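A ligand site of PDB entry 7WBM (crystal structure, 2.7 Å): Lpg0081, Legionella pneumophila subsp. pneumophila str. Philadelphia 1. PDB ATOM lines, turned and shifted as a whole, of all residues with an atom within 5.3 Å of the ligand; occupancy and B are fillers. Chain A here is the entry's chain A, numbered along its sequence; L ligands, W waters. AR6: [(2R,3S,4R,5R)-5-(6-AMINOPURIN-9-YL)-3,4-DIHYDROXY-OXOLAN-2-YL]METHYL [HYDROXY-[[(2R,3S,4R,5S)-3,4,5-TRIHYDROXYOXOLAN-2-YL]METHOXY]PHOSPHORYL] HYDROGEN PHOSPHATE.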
ATOM      1  N   ASN A  61       5.503  16.310  32.479  1.00  0.00           N
ATOM      2  CA  ASN A  61       5.336  15.570  33.728  1.00  0.00           C
ATOM      3  C   ASN A  61       4.574  14.279  33.453  1.00  0.00           C
ATOM      4  O   ASN A  61       3.438  14.329  32.964  1.00  0.00           O
ATOM      5  CB  ASN A  61       4.605  16.405  34.786  1.00  0.00           C
ATOM      6  CG  ASN A  61       4.717  15.827  36.190  1.00  0.00           C
ATOM      7  OD1 ASN A  61       4.740  14.608  36.370  1.00  0.00           O
ATOM      8  ND2 ASN A  61       4.768  16.695  37.201  1.00  0.00           N
ATOM      9  N   VAL A  62       5.170  13.140  33.753  1.00  0.00           N
ATOM     10  CA  VAL A  62       4.463  11.866  33.702  1.00  0.00           C
ATOM     11  C   VAL A  62       4.833  11.067  34.928  1.00  0.00           C
ATOM     12  O   VAL A  62       5.734  11.421  35.693  1.00  0.00           O
ATOM     13  CB  VAL A  62       4.757  11.051  32.433  1.00  0.00           C
ATOM     14  CG1 VAL A  62       3.937  11.609  31.233  1.00  0.00           C
ATOM     15  CG2 VAL A  62       6.294  10.971  32.188  1.00  0.00           C
ATOM     16  N   TYR A 119      -2.666   7.947  19.294  1.00  0.00           N
ATOM     17  CA  TYR A 119      -2.494   7.306  20.610  1.00  0.00           C
ATOM     18  C   TYR A 119      -3.759   6.535  20.989  1.00  0.00           C
ATOM     19  O   TYR A 119      -4.873   7.071  20.879  1.00  0.00           O
ATOM     20  CB  TYR A 119      -2.160   8.335  21.698  1.00  0.00           C
ATOM     21  CG  TYR A 119      -2.139   7.713  23.065  1.00  0.00           C
ATOM     22  CD1 TYR A 119      -3.304   7.611  23.829  1.00  0.00           C
ATOM     23  CD2 TYR A 119      -0.955   7.188  23.597  1.00  0.00           C
ATOM     24  CE1 TYR A 119      -3.286   7.014  25.071  1.00  0.00           C
ATOM     25  CE2 TYR A 119      -0.937   6.591  24.839  1.00  0.00           C
ATOM     26  CZ  TYR A 119      -2.098   6.507  25.561  1.00  0.00           C
ATOM     27  OH  TYR A 119      -2.080   5.931  26.811  1.00  0.00           O
ATOM     28  N   PRO A 120      -3.629   5.285  21.441  1.00  0.00           N
ATOM     29  CA  PRO A 120      -2.354   4.540  21.491  1.00  0.00           C
ATOM     30  C   PRO A 120      -1.818   4.030  20.128  1.00  0.00           C
ATOM     31  O   PRO A 120      -2.362   4.336  19.073  1.00  0.00           O
ATOM     32  CB  PRO A 120      -2.684   3.341  22.385  1.00  0.00           C
ATOM     33  CG  PRO A 120      -4.170   3.322  22.546  1.00  0.00           C
ATOM     34  CD  PRO A 120      -4.778   4.534  21.960  1.00  0.00           C
ATOM     35  N   ASN A 123      -3.920   2.999  17.271  1.00  0.00           N
ATOM     36  CA  ASN A 123      -4.930   3.938  16.775  1.00  0.00           C
ATOM     37  C   ASN A 123      -4.279   4.841  15.733  1.00  0.00           C
ATOM     38  O   ASN A 123      -3.575   5.804  16.088  1.00  0.00           O
ATOM     39  CB  ASN A 123      -5.514   4.768  17.932  1.00  0.00           C
ATOM     40  CG  ASN A 123      -6.392   5.911  17.454  1.00  0.00           C
ATOM     41  OD1 ASN A 123      -6.980   5.876  16.362  1.00  0.00           O
ATOM     42  ND2 ASN A 123      -6.486   6.948  18.279  1.00  0.00           N
ATOM     43  N   GLY A 141      -8.422  15.572  35.478  1.00  0.00           N
ATOM     44  CA  GLY A 141      -9.199  14.745  36.375  1.00  0.00           C
ATOM     45  C   GLY A 141      -8.417  14.511  37.647  1.00  0.00           C
ATOM     46  O   GLY A 141      -7.246  14.889  37.774  1.00  0.00           O
ATOM     47  N   GLU A 145      -1.796   8.838  40.590  1.00  0.00           N
ATOM     48  CA  GLU A 145      -0.482   8.300  40.224  1.00  0.00           C
ATOM     49  C   GLU A 145       0.492   8.343  41.392  1.00  0.00           C
ATOM     50  O   GLU A 145       1.432   7.536  41.448  1.00  0.00           O
ATOM     51  CB  GLU A 145       0.105   9.054  39.027  1.00  0.00           C
ATOM     52  CG  GLU A 145      -0.543   8.753  37.678  1.00  0.00           C
ATOM     53  CD  GLU A 145       0.247   9.358  36.506  1.00  0.00           C
ATOM     54  OE1 GLU A 145       0.720   8.615  35.610  1.00  0.00           O
ATOM     55  OE2 GLU A 145       0.387  10.582  36.482  1.00  0.00           O
ATOM     56  N   THR A 261     -14.426  12.571  26.619  1.00  0.00           N
ATOM     57  CA  THR A 261     -13.265  11.757  26.952  1.00  0.00           C
ATOM     58  C   THR A 261     -13.353  11.183  28.363  1.00  0.00           C
ATOM     59  O   THR A 261     -13.910  11.815  29.266  1.00  0.00           O
ATOM     60  CB  THR A 261     -12.003  12.607  26.807  1.00  0.00           C
ATOM     61  OG1 THR A 261     -12.191  13.508  25.714  1.00  0.00           O
ATOM     62  CG2 THR A 261     -10.786  11.726  26.524  1.00  0.00           C
ATOM     63  N   ALA A 262     -12.817   9.987  28.565  1.00  0.00           N
ATOM     64  CA  ALA A 262     -12.817   9.392  29.901  1.00  0.00           C
ATOM     65  C   ALA A 262     -11.675   9.990  30.732  1.00  0.00           C
ATOM     66  O   ALA A 262     -10.667   9.334  31.029  1.00  0.00           O
ATOM     67  CB  ALA A 262     -12.736   7.874  29.781  1.00  0.00           C
ATOM     68  N   VAL A 263     -11.833  11.272  31.105  1.00  0.00           N
ATOM     69  CA  VAL A 263     -10.874  11.964  31.969  1.00  0.00           C
ATOM     70  C   VAL A 263     -10.595  11.127  33.201  1.00  0.00           C
ATOM     71  O   VAL A 263     -11.513  10.740  33.925  1.00  0.00           O
ATOM     72  CB  VAL A 263     -11.425  13.323  32.444  1.00  0.00           C
ATOM     73  CG1 VAL A 263     -10.276  14.243  32.872  1.00  0.00           C
ATOM     74  CG2 VAL A 263     -12.315  13.949  31.434  1.00  0.00           C
ATOM     75  N   GLY A 264      -9.320  10.897  33.490  1.00  0.00           N
ATOM     76  CA  GLY A 264      -8.910  10.277  34.719  1.00  0.00           C
ATOM     77  C   GLY A 264      -8.849   8.770  34.709  1.00  0.00           C
ATOM     78  O   GLY A 264      -8.422   8.184  35.711  1.00  0.00           O
ATOM     79  N   MET A 265      -9.230   8.126  33.606  1.00  0.00           N
ATOM     80  CA  MET A 265      -9.430   6.681  33.634  1.00  0.00           C
ATOM     81  C   MET A 265      -8.268   5.915  33.023  1.00  0.00           C
ATOM     82  O   MET A 265      -8.356   4.688  32.886  1.00  0.00           O
ATOM     83  CB  MET A 265     -10.733   6.307  32.936  1.00  0.00           C
ATOM     84  CG  MET A 265     -11.948   7.102  33.398  1.00  0.00           C
ATOM     85  SD  MET A 265     -12.308   6.886  35.156  1.00  0.00           S
ATOM     86  CE  MET A 265     -13.017   8.504  35.475  1.00  0.00           C
ATOM     87  N   GLY A 266      -7.199   6.624  32.665  1.00  0.00           N
ATOM     88  CA  GLY A 266      -6.013   6.061  32.068  1.00  0.00           C
ATOM     89  C   GLY A 266      -4.860   6.103  33.040  1.00  0.00           C
ATOM     90  O   GLY A 266      -4.825   5.349  34.011  1.00  0.00           O
ATOM     91  N   PHE A 267      -3.897   6.994  32.800  1.00  0.00           N
ATOM     92  CA  PHE A 267      -2.734   7.072  33.674  1.00  0.00           C
ATOM     93  C   PHE A 267      -3.139   7.442  35.104  1.00  0.00           C
ATOM     94  O   PHE A 267      -2.690   6.816  36.065  1.00  0.00           O
ATOM     95  CB  PHE A 267      -1.730   8.071  33.124  1.00  0.00           C
ATOM     96  CG  PHE A 267      -1.105   7.635  31.823  1.00  0.00           C
ATOM     97  CD1 PHE A 267      -0.125   6.647  31.805  1.00  0.00           C
ATOM     98  CD2 PHE A 267      -1.479   8.245  30.618  1.00  0.00           C
ATOM     99  CE1 PHE A 267       0.487   6.257  30.608  1.00  0.00           C
ATOM    100  CE2 PHE A 267      -0.872   7.845  29.400  1.00  0.00           C
ATOM    101  CZ  PHE A 267       0.110   6.856  29.396  1.00  0.00           C
ATOM    102  N   PHE A 268      -3.981   8.451  35.239  1.00  0.00           N
ATOM    103  CA  PHE A 268      -4.406   8.925  36.552  1.00  0.00           C
ATOM    104  C   PHE A 268      -5.112   7.842  37.364  1.00  0.00           C
ATOM    105  O   PHE A 268      -5.277   8.010  38.584  1.00  0.00           O
ATOM    106  CB  PHE A 268      -5.328  10.153  36.398  1.00  0.00           C
ATOM    107  CG  PHE A 268      -4.595  11.469  36.179  1.00  0.00           C
ATOM    108  CD1 PHE A 268      -3.232  11.506  35.903  1.00  0.00           C
ATOM    109  CD2 PHE A 268      -5.276  12.670  36.255  1.00  0.00           C
ATOM    110  CE1 PHE A 268      -2.586  12.705  35.726  1.00  0.00           C
ATOM    111  CE2 PHE A 268      -4.618  13.876  36.063  1.00  0.00           C
ATOM    112  CZ  PHE A 268      -3.266  13.886  35.794  1.00  0.00           C
ATOM    113  N   ALA A 269      -5.592   6.775  36.737  1.00  0.00           N
ATOM    114  CA  ALA A 269      -6.362   5.755  37.446  1.00  0.00           C
ATOM    115  C   ALA A 269      -5.499   4.654  38.065  1.00  0.00           C
ATOM    116  O   ALA A 269      -6.030   3.776  38.769  1.00  0.00           O
ATOM    117  CB  ALA A 269      -7.392   5.130  36.502  1.00  0.00           C
ATOM    118  N   PRO A 307     -16.323   8.258  24.359  1.00  0.00           N
ATOM    119  CA  PRO A 307     -15.397   7.272  23.776  1.00  0.00           C
ATOM    120  C   PRO A 307     -15.011   6.220  24.810  1.00  0.00           C
ATOM    121  O   PRO A 307     -14.338   6.530  25.793  1.00  0.00           O
ATOM    122  CB  PRO A 307     -14.193   8.123  23.331  1.00  0.00           C
ATOM    123  CG  PRO A 307     -14.643   9.587  23.462  1.00  0.00           C
ATOM    124  CD  PRO A 307     -15.691   9.570  24.556  1.00  0.00           C
ATOM    125  N   PHE A 309     -13.629   2.178  25.160  1.00  0.00           N
ATOM    126  CA  PHE A 309     -12.994   1.090  24.427  1.00  0.00           C
ATOM    127  C   PHE A 309     -12.845  -0.205  25.223  1.00  0.00           C
ATOM    128  O   PHE A 309     -12.408  -1.210  24.666  1.00  0.00           O
ATOM    129  CB  PHE A 309     -11.605   1.525  23.916  1.00  0.00           C
ATOM    130  CG  PHE A 309     -11.607   2.882  23.289  1.00  0.00           C
ATOM    131  CD1 PHE A 309     -11.496   4.029  24.080  1.00  0.00           C
ATOM    132  CD2 PHE A 309     -11.732   3.016  21.922  1.00  0.00           C
ATOM    133  CE1 PHE A 309     -11.511   5.297  23.512  1.00  0.00           C
ATOM    134  CE2 PHE A 309     -11.748   4.299  21.318  1.00  0.00           C
ATOM    135  CZ  PHE A 309     -11.635   5.445  22.124  1.00  0.00           C
ATOM    136  N   GLN A 313     -16.252  -0.940  30.979  1.00  0.00           N
ATOM    137  CA  GLN A 313     -16.856   0.386  30.915  1.00  0.00           C
ATOM    138  C   GLN A 313     -18.036   0.409  29.952  1.00  0.00           C
ATOM    139  O   GLN A 313     -18.999   1.151  30.170  1.00  0.00           O
ATOM    140  CB  GLN A 313     -15.831   1.425  30.467  1.00  0.00           C
ATOM    141  CG  GLN A 313     -14.511   1.467  31.180  1.00  0.00           C
ATOM    142  CD  GLN A 313     -13.538   2.488  30.521  1.00  0.00           C
ATOM    143  OE1 GLN A 313     -13.477   2.606  29.291  1.00  0.00           O
ATOM    144  NE2 GLN A 313     -12.775   3.223  31.358  1.00  0.00           N
ATOM    145  N   ARG A 335     -14.799   5.783  18.717  1.00  0.00           N
ATOM    146  CA  ARG A 335     -14.233   6.717  17.757  1.00  0.00           C
ATOM    147  C   ARG A 335     -13.263   7.637  18.488  1.00  0.00           C
ATOM    148  O   ARG A 335     -13.508   8.075  19.617  1.00  0.00           O
ATOM    149  CB  ARG A 335     -15.340   7.530  17.076  1.00  0.00           C
ATOM    150  CG  ARG A 335     -14.825   8.586  16.103  1.00  0.00           C
ATOM    151  CD  ARG A 335     -15.933   9.143  15.188  1.00  0.00           C
ATOM    152  NE  ARG A 335     -16.997   9.839  15.912  1.00  0.00           N
ATOM    153  CZ  ARG A 335     -17.888  10.650  15.345  1.00  0.00           C
ATOM    154  NH1 ARG A 335     -17.844  10.888  14.047  1.00  0.00           N
ATOM    155  NH2 ARG A 335     -18.803  11.252  16.089  1.00  0.00           N
ATOM    156  N   ASP A 336     -12.142   7.935  17.830  1.00  0.00           N
ATOM    157  CA  ASP A 336     -11.140   8.810  18.404  1.00  0.00           C
ATOM    158  C   ASP A 336     -11.751  10.153  18.813  1.00  0.00           C
ATOM    159  O   ASP A 336     -12.632  10.680  18.115  1.00  0.00           O
ATOM    160  CB  ASP A 336     -10.019   8.998  17.402  1.00  0.00           C
ATOM    161  CG  ASP A 336      -8.905   9.836  17.941  1.00  0.00           C
ATOM    162  OD1 ASP A 336      -8.029   9.264  18.629  1.00  0.00           O
ATOM    163  OD2 ASP A 336      -8.902  11.054  17.673  1.00  0.00           O
ATOM    164  N   VAL A 337     -11.302  10.678  19.957  1.00  0.00           N
ATOM    165  CA  VAL A 337     -11.793  11.943  20.519  1.00  0.00           C
ATOM    166  C   VAL A 337     -11.870  13.040  19.451  1.00  0.00           C
ATOM    167  O   VAL A 337     -12.858  13.795  19.387  1.00  0.00           O
ATOM    168  CB  VAL A 337     -10.955  12.392  21.732  1.00  0.00           C
ATOM    169  CG1 VAL A 337      -9.500  12.673  21.366  1.00  0.00           C
ATOM    170  CG2 VAL A 337     -11.560  13.611  22.373  1.00  0.00           C
ATOM    171  N   PRO A 355      -8.161  15.476  28.353  1.00  0.00           N
ATOM    172  CA  PRO A 355      -7.797  15.007  29.705  1.00  0.00           C
ATOM    173  C   PRO A 355      -6.392  15.465  30.050  1.00  0.00           C
ATOM    174  O   PRO A 355      -5.419  14.892  29.537  1.00  0.00           O
ATOM    175  CB  PRO A 355      -7.912  13.482  29.604  1.00  0.00           C
ATOM    176  CG  PRO A 355      -7.660  13.167  28.186  1.00  0.00           C
ATOM    177  CD  PRO A 355      -8.067  14.393  27.360  1.00  0.00           C
ATOM    178  N   SER A 356      -6.287  16.507  30.884  1.00  0.00           N
ATOM    179  CA  SER A 356      -5.056  17.277  31.028  1.00  0.00           C
ATOM    180  C   SER A 356      -4.400  17.066  32.400  1.00  0.00           C
ATOM    181  O   SER A 356      -4.796  16.191  33.184  1.00  0.00           O
ATOM    182  CB  SER A 356      -5.337  18.750  30.744  1.00  0.00           C
ATOM    183  OG  SER A 356      -4.126  19.430  30.484  1.00  0.00           O
ATOM    184  N   ASP A 357      -3.385  17.896  32.671  1.00  0.00           N
ATOM    185  CA  ASP A 357      -2.594  17.890  33.888  1.00  0.00           C
ATOM    186  C   ASP A 357      -2.617  19.274  34.506  1.00  0.00           C
ATOM    187  O   ASP A 357      -2.310  20.266  33.811  1.00  0.00           O
ATOM    188  CB  ASP A 357      -1.129  17.480  33.603  1.00  0.00           C
ATOM    189  CG  ASP A 357      -0.452  16.822  34.795  1.00  0.00           C
ATOM    190  OD1 ASP A 357      -0.493  17.342  35.945  1.00  0.00           O
ATOM    191  OD2 ASP A 357       0.120  15.733  34.589  1.00  0.00           O
ATOM    192  N   ASN A 364       1.416  18.787  27.479  1.00  0.00           N
ATOM    193  CA  ASN A 364       2.348  17.919  28.201  1.00  0.00           C
ATOM    194  C   ASN A 364       3.403  17.287  27.284  1.00  0.00           C
ATOM    195  O   ASN A 364       4.124  18.004  26.577  1.00  0.00           O
ATOM    196  CB  ASN A 364       1.589  16.850  28.992  1.00  0.00           C
ATOM    197  CG  ASN A 364       2.362  16.376  30.246  1.00  0.00           C
ATOM    198  OD1 ASN A 364       3.582  16.465  30.323  1.00  0.00           O
ATOM    199  ND2 ASN A 364       1.621  15.887  31.251  1.00  0.00           N
ATOM    200  N   GLU A 365       3.486  15.951  27.285  1.00  0.00           N
ATOM    201  CA  GLU A 365       4.519  15.248  26.521  1.00  0.00           C
ATOM    202  C   GLU A 365       4.504  15.635  25.042  1.00  0.00           C
ATOM    203  O   GLU A 365       3.485  16.015  24.467  1.00  0.00           O
ATOM    204  CB  GLU A 365       4.339  13.728  26.612  1.00  0.00           C
ATOM    205  CG  GLU A 365       4.810  13.136  27.901  1.00  0.00           C
ATOM    206  CD  GLU A 365       4.542  11.652  27.940  1.00  0.00           C
ATOM    207  OE1 GLU A 365       3.382  11.275  28.211  1.00  0.00           O
ATOM    208  OE2 GLU A 365       5.486  10.861  27.698  1.00  0.00           O
ATOM    209  N   SER A 370      -0.002  10.050  25.302  1.00  0.00           N
ATOM    210  CA  SER A 370      -1.208  10.145  26.107  1.00  0.00           C
ATOM    211  C   SER A 370      -2.251  10.790  25.228  1.00  0.00           C
ATOM    212  O   SER A 370      -1.933  11.350  24.178  1.00  0.00           O
ATOM    213  CB  SER A 370      -0.992  10.972  27.391  1.00  0.00           C
ATOM    214  OG  SER A 370      -0.454  12.242  27.066  1.00  0.00           O
ATOM    215  N   VAL A 371      -3.496  10.798  25.710  1.00  0.00           N
ATOM    216  CA  VAL A 371      -4.558  11.474  24.963  1.00  0.00           C
ATOM    217  C   VAL A 371      -4.245  12.965  24.842  1.00  0.00           C
ATOM    218  O   VAL A 371      -4.305  13.539  23.746  1.00  0.00           O
ATOM    219  CB  VAL A 371      -5.930  11.238  25.602  1.00  0.00           C
ATOM    220  CG1 VAL A 371      -7.026  11.829  24.724  1.00  0.00           C
ATOM    221  CG2 VAL A 371      -6.223   9.719  25.847  1.00  0.00           C
ATOM    222  N   GLU A 372      -3.838  13.600  25.935  1.00  0.00           N
ATOM    223  CA  GLU A 372      -3.506  15.017  25.863  1.00  0.00           C
ATOM    224  C   GLU A 372      -2.370  15.284  24.880  1.00  0.00           C
ATOM    225  O   GLU A 372      -2.485  16.155  24.019  1.00  0.00           O
ATOM    226  CB  GLU A 372      -3.123  15.573  27.252  1.00  0.00           C
ATOM    227  CG  GLU A 372      -2.432  16.948  27.120  1.00  0.00           C
ATOM    228  CD  GLU A 372      -2.549  17.782  28.387  1.00  0.00           C
ATOM    229  OE1 GLU A 372      -2.278  17.252  29.480  1.00  0.00           O
ATOM    230  OE2 GLU A 372      -2.885  18.972  28.286  1.00  0.00           O
ATOM    231  N   MET A 374      -1.356  13.546  22.426  1.00  0.00           N
ATOM    232  CA  MET A 374      -1.915  13.367  21.092  1.00  0.00           C
ATOM    233  C   MET A 374      -2.668  14.615  20.623  1.00  0.00           C
ATOM    234  O   MET A 374      -2.423  15.120  19.519  1.00  0.00           O
ATOM    235  CB  MET A 374      -2.849  12.161  21.069  1.00  0.00           C
ATOM    236  CG  MET A 374      -3.555  12.000  19.723  1.00  0.00           C
ATOM    237  SD  MET A 374      -4.859  10.767  19.841  1.00  0.00           S
ATOM    238  CE  MET A 374      -5.904  11.552  21.062  1.00  0.00           C
HETATM  239  N1  AR6 L   1      -9.543   8.859  21.927  1.00  0.00           N
HETATM  240  C2  AR6 L   1     -10.449   9.041  22.937  1.00  0.00           C
HETATM  241  N3  AR6 L   1     -10.223   8.455  24.158  1.00  0.00           N
HETATM  242  C4  AR6 L   1      -9.123   7.716  24.383  1.00  0.00           C
HETATM  243  C5  AR6 L   1      -8.219   7.542  23.388  1.00  0.00           C
HETATM  244  C6  AR6 L   1      -8.447   8.129  22.152  1.00  0.00           C
HETATM  245  N6  AR6 L   1      -7.713   8.127  20.953  1.00  0.00           N
HETATM  246  N7  AR6 L   1      -7.207   6.772  23.839  1.00  0.00           N
HETATM  247  C8  AR6 L   1      -7.488   6.472  25.113  1.00  0.00           C
HETATM  248  N9  AR6 L   1      -8.674   7.053  25.462  1.00  0.00           N
HETATM  249  PA  AR6 L   1      -5.189   9.378  29.523  1.00  0.00           P
HETATM  250  PB  AR6 L   1      -5.797  10.569  32.122  1.00  0.00           P
HETATM  251  C1' AR6 L   1      -9.311   6.999  26.740  1.00  0.00           C
HETATM  252  O1A AR6 L   1      -4.327   9.895  28.423  1.00  0.00           O
HETATM  253  O1B AR6 L   1      -6.069   9.180  32.803  1.00  0.00           O
HETATM  254  C1D AR6 L   1      -1.472  12.855  30.366  1.00  0.00           C
HETATM  255  O1D AR6 L   1      -0.219  12.762  30.255  1.00  0.00           O
HETATM  256  C2' AR6 L   1      -8.946   5.904  27.416  1.00  0.00           C
HETATM  257  O2' AR6 L   1     -10.165   5.232  27.955  1.00  0.00           O
HETATM  258  O2A AR6 L   1      -4.509   8.308  30.255  1.00  0.00           O
HETATM  259  O2B AR6 L   1      -6.832  11.560  32.474  1.00  0.00           O
HETATM  260  C2D AR6 L   1      -1.853  14.200  30.995  1.00  0.00           C
HETATM  261  O2D AR6 L   1      -0.866  15.188  30.574  1.00  0.00           O
HETATM  262  C3' AR6 L   1      -8.037   6.412  28.563  1.00  0.00           C
HETATM  263  O3' AR6 L   1      -8.035   5.581  29.609  1.00  0.00           O
HETATM  264  O3A AR6 L   1      -5.783  10.545  30.458  1.00  0.00           O
HETATM  265  C3D AR6 L   1      -1.830  13.953  32.327  1.00  0.00           C
HETATM  266  O3D AR6 L   1      -0.545  13.912  32.802  1.00  0.00           O
HETATM  267  C4' AR6 L   1      -8.733   7.782  28.903  1.00  0.00           C
HETATM  268  O4' AR6 L   1      -8.905   8.278  27.712  1.00  0.00           O
HETATM  269  C4D AR6 L   1      -2.422  12.413  32.451  1.00  0.00           C
HETATM  270  O4D AR6 L   1      -2.033  11.753  31.391  1.00  0.00           O
HETATM  271  C5' AR6 L   1      -7.726   8.608  29.716  1.00  0.00           C
HETATM  272  O5' AR6 L   1      -6.578   8.770  28.844  1.00  0.00           O
HETATM  273  C5D AR6 L   1      -3.917  12.387  32.548  1.00  0.00           C
HETATM  274  O5D AR6 L   1      -4.294  11.031  32.679  1.00  0.00           O
HETATM  275  O   HOH W   1       1.449  13.503  28.500  1.00  0.00           O
HETATM  276  O   HOH W   2      -9.909   4.087  31.047  1.00  0.00           O
HETATM  277  O   HOH W   3     -12.428   8.697  26.222  1.00  0.00           O
HETATM  278  O   HOH W   4      -6.686  14.048  33.439  1.00  0.00           O
HETATM  279  O   HOH W   5       0.827  10.282  31.674  1.00  0.00           O
HETATM  280  O   HOH W   6      -3.812  12.577  28.311  1.00  0.00           O
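The backbone NH (N) of Val 371 sits at hydrogen-bond distance from an oxygen (O1A) of the ligand, 3.0 Å away. ND2 of Asn 364 is in hydrogen-bond range of O2D of the ligand, at 2.7 Å. ND2 of Asn 123 lies close to N6 of the ligand (3.2 Å). An oxygen (O2A) of the ligand is in hydrogen-bond range of the backbone NH (N) of Phe 267, 2.9 Å away. The backbone NH (N) of Val 337 lies within hydrogen-bond range of a nitrogen (N1) of the ligand. The backbone NH (N) of Met 265 sits at hydrogen-bond distance from an oxygen (O1B) of the ligand, at 3.4 Å. O of Tyr 119 lies within hydrogen-bond range of N6 of the ligand, at 3.0 Å. OD2 of Asp 357 sits at hydrogen-bond distance from O3D of the ligand, at 2.6 Å. An oxygen (O2B) of the ligand sits at hydrogen-bond distance from the backbone NH (N) of Gly 264, at 2.8 Å. A nitrogen (N6) of the ligand is in hydrogen-bond range of the side-chain carboxylate of Asp 336 (2.6 Å). The side-chain hydroxyl (OG) of Ser 370 lies within hydrogen-bond range of an oxygen (O1D) of the ligand (3.2 Å). The backbone NH (N) of Gly 266 sits at hydrogen-bond distance from an oxygen (O1B) of the ligand, 2.8 Å away. The side-chain carboxylate (OE1) of Glu 372 is in hydrogen-bond range of an oxygen (O2D) of the ligand. The backbone NH of Phe 268 sits at hydrogen-bond distance from an oxygen (O1B) of the ligand, 3.3 Å away. The backbone carbonyl oxygen (O) of Met 265 is in hydrogen-bond range of an oxygen (O3') of the ligand (3.4 Å).
OE2 of Glu 372 sits at hydrogen-bond distance from OG of Ser 356 (2.6 Å). The backbone carbonyl oxygen (O) of Gly 264 sits close to the backbone NH (N) of Ala 269. SD of Met 374 lies within hydrogen-bond range of N of Tyr 119 (3.6 Å). OD1 of Asn 364 sits at hydrogen-bond distance from N of Asn 61 (2.9 Å). The backbone carbonyl oxygen (O) of Tyr 119 is in hydrogen-bond range of the side-chain amide nitrogen (ND2) of Asn 123 (3.1 Å). The side-chain amide nitrogen (ND2) of Asn 123 is in hydrogen-bond range of the side-chain carboxylate (OD1) of Asp 336, 2.8 Å away. OE1 of Glu 372 lies within hydrogen-bond range of N of Asp 357, 3.4 Å away.
Residues that only touch the ligand: Ala 262 (3.3 Å), Phe 309 (3.5 Å), Pro 355 (3.6 Å), Pro 120 (3.8 Å), Ser 356 (3.8 Å), Val 263 (3.9 Å), Met 374 (3.9 Å) and Pro 307 (3.9 Å). Hydrophobic or aromatic side chains that line the ligand: Tyr 119, Pro 120, Phe 267, Phe 268, Pro 307, Phe 309, Val 337, Pro 355, Val 371 and Met 374. Of the 31 residues printed, 22 come within 4 Å of the ligand. The nearest printed residue that does not touch the ligand is Asn 61 (4.01 Å).
Water W1 lies within hydrogen-bond range of an oxygen (O1D) of the ligand (2.5 Å), the side-chain hydroxyl (OG) of Ser 370 (2.7 Å) and the side-chain carboxylate (OE1) of Glu 365 (3.0 Å). Water W4 lies within hydrogen-bond range of O2B of the ligand (2.7 Å), O of Ser 356 (2.9 Å) and N of Gly 141 (3.1 Å). Water W6 lies within hydrogen-bond range of N of Glu 372 (2.6 Å), O1A of the ligand (2.7 Å), O of Pro 355 (3.1 Å) and N of Val 371 (3.2 Å). Water W2 lies within hydrogen-bond range of the backbone carbonyl oxygen (O) of Met 265 (2.5 Å), an oxygen (O3') of the ligand (2.8 Å) and the side-chain amide nitrogen (NE2) of Gln 313 (3.0 Å). Water W3 lies within hydrogen-bond range of the backbone NH of Ala 262, the backbone carbonyl oxygen of Pro 307 and a nitrogen (N3) of the ligand.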
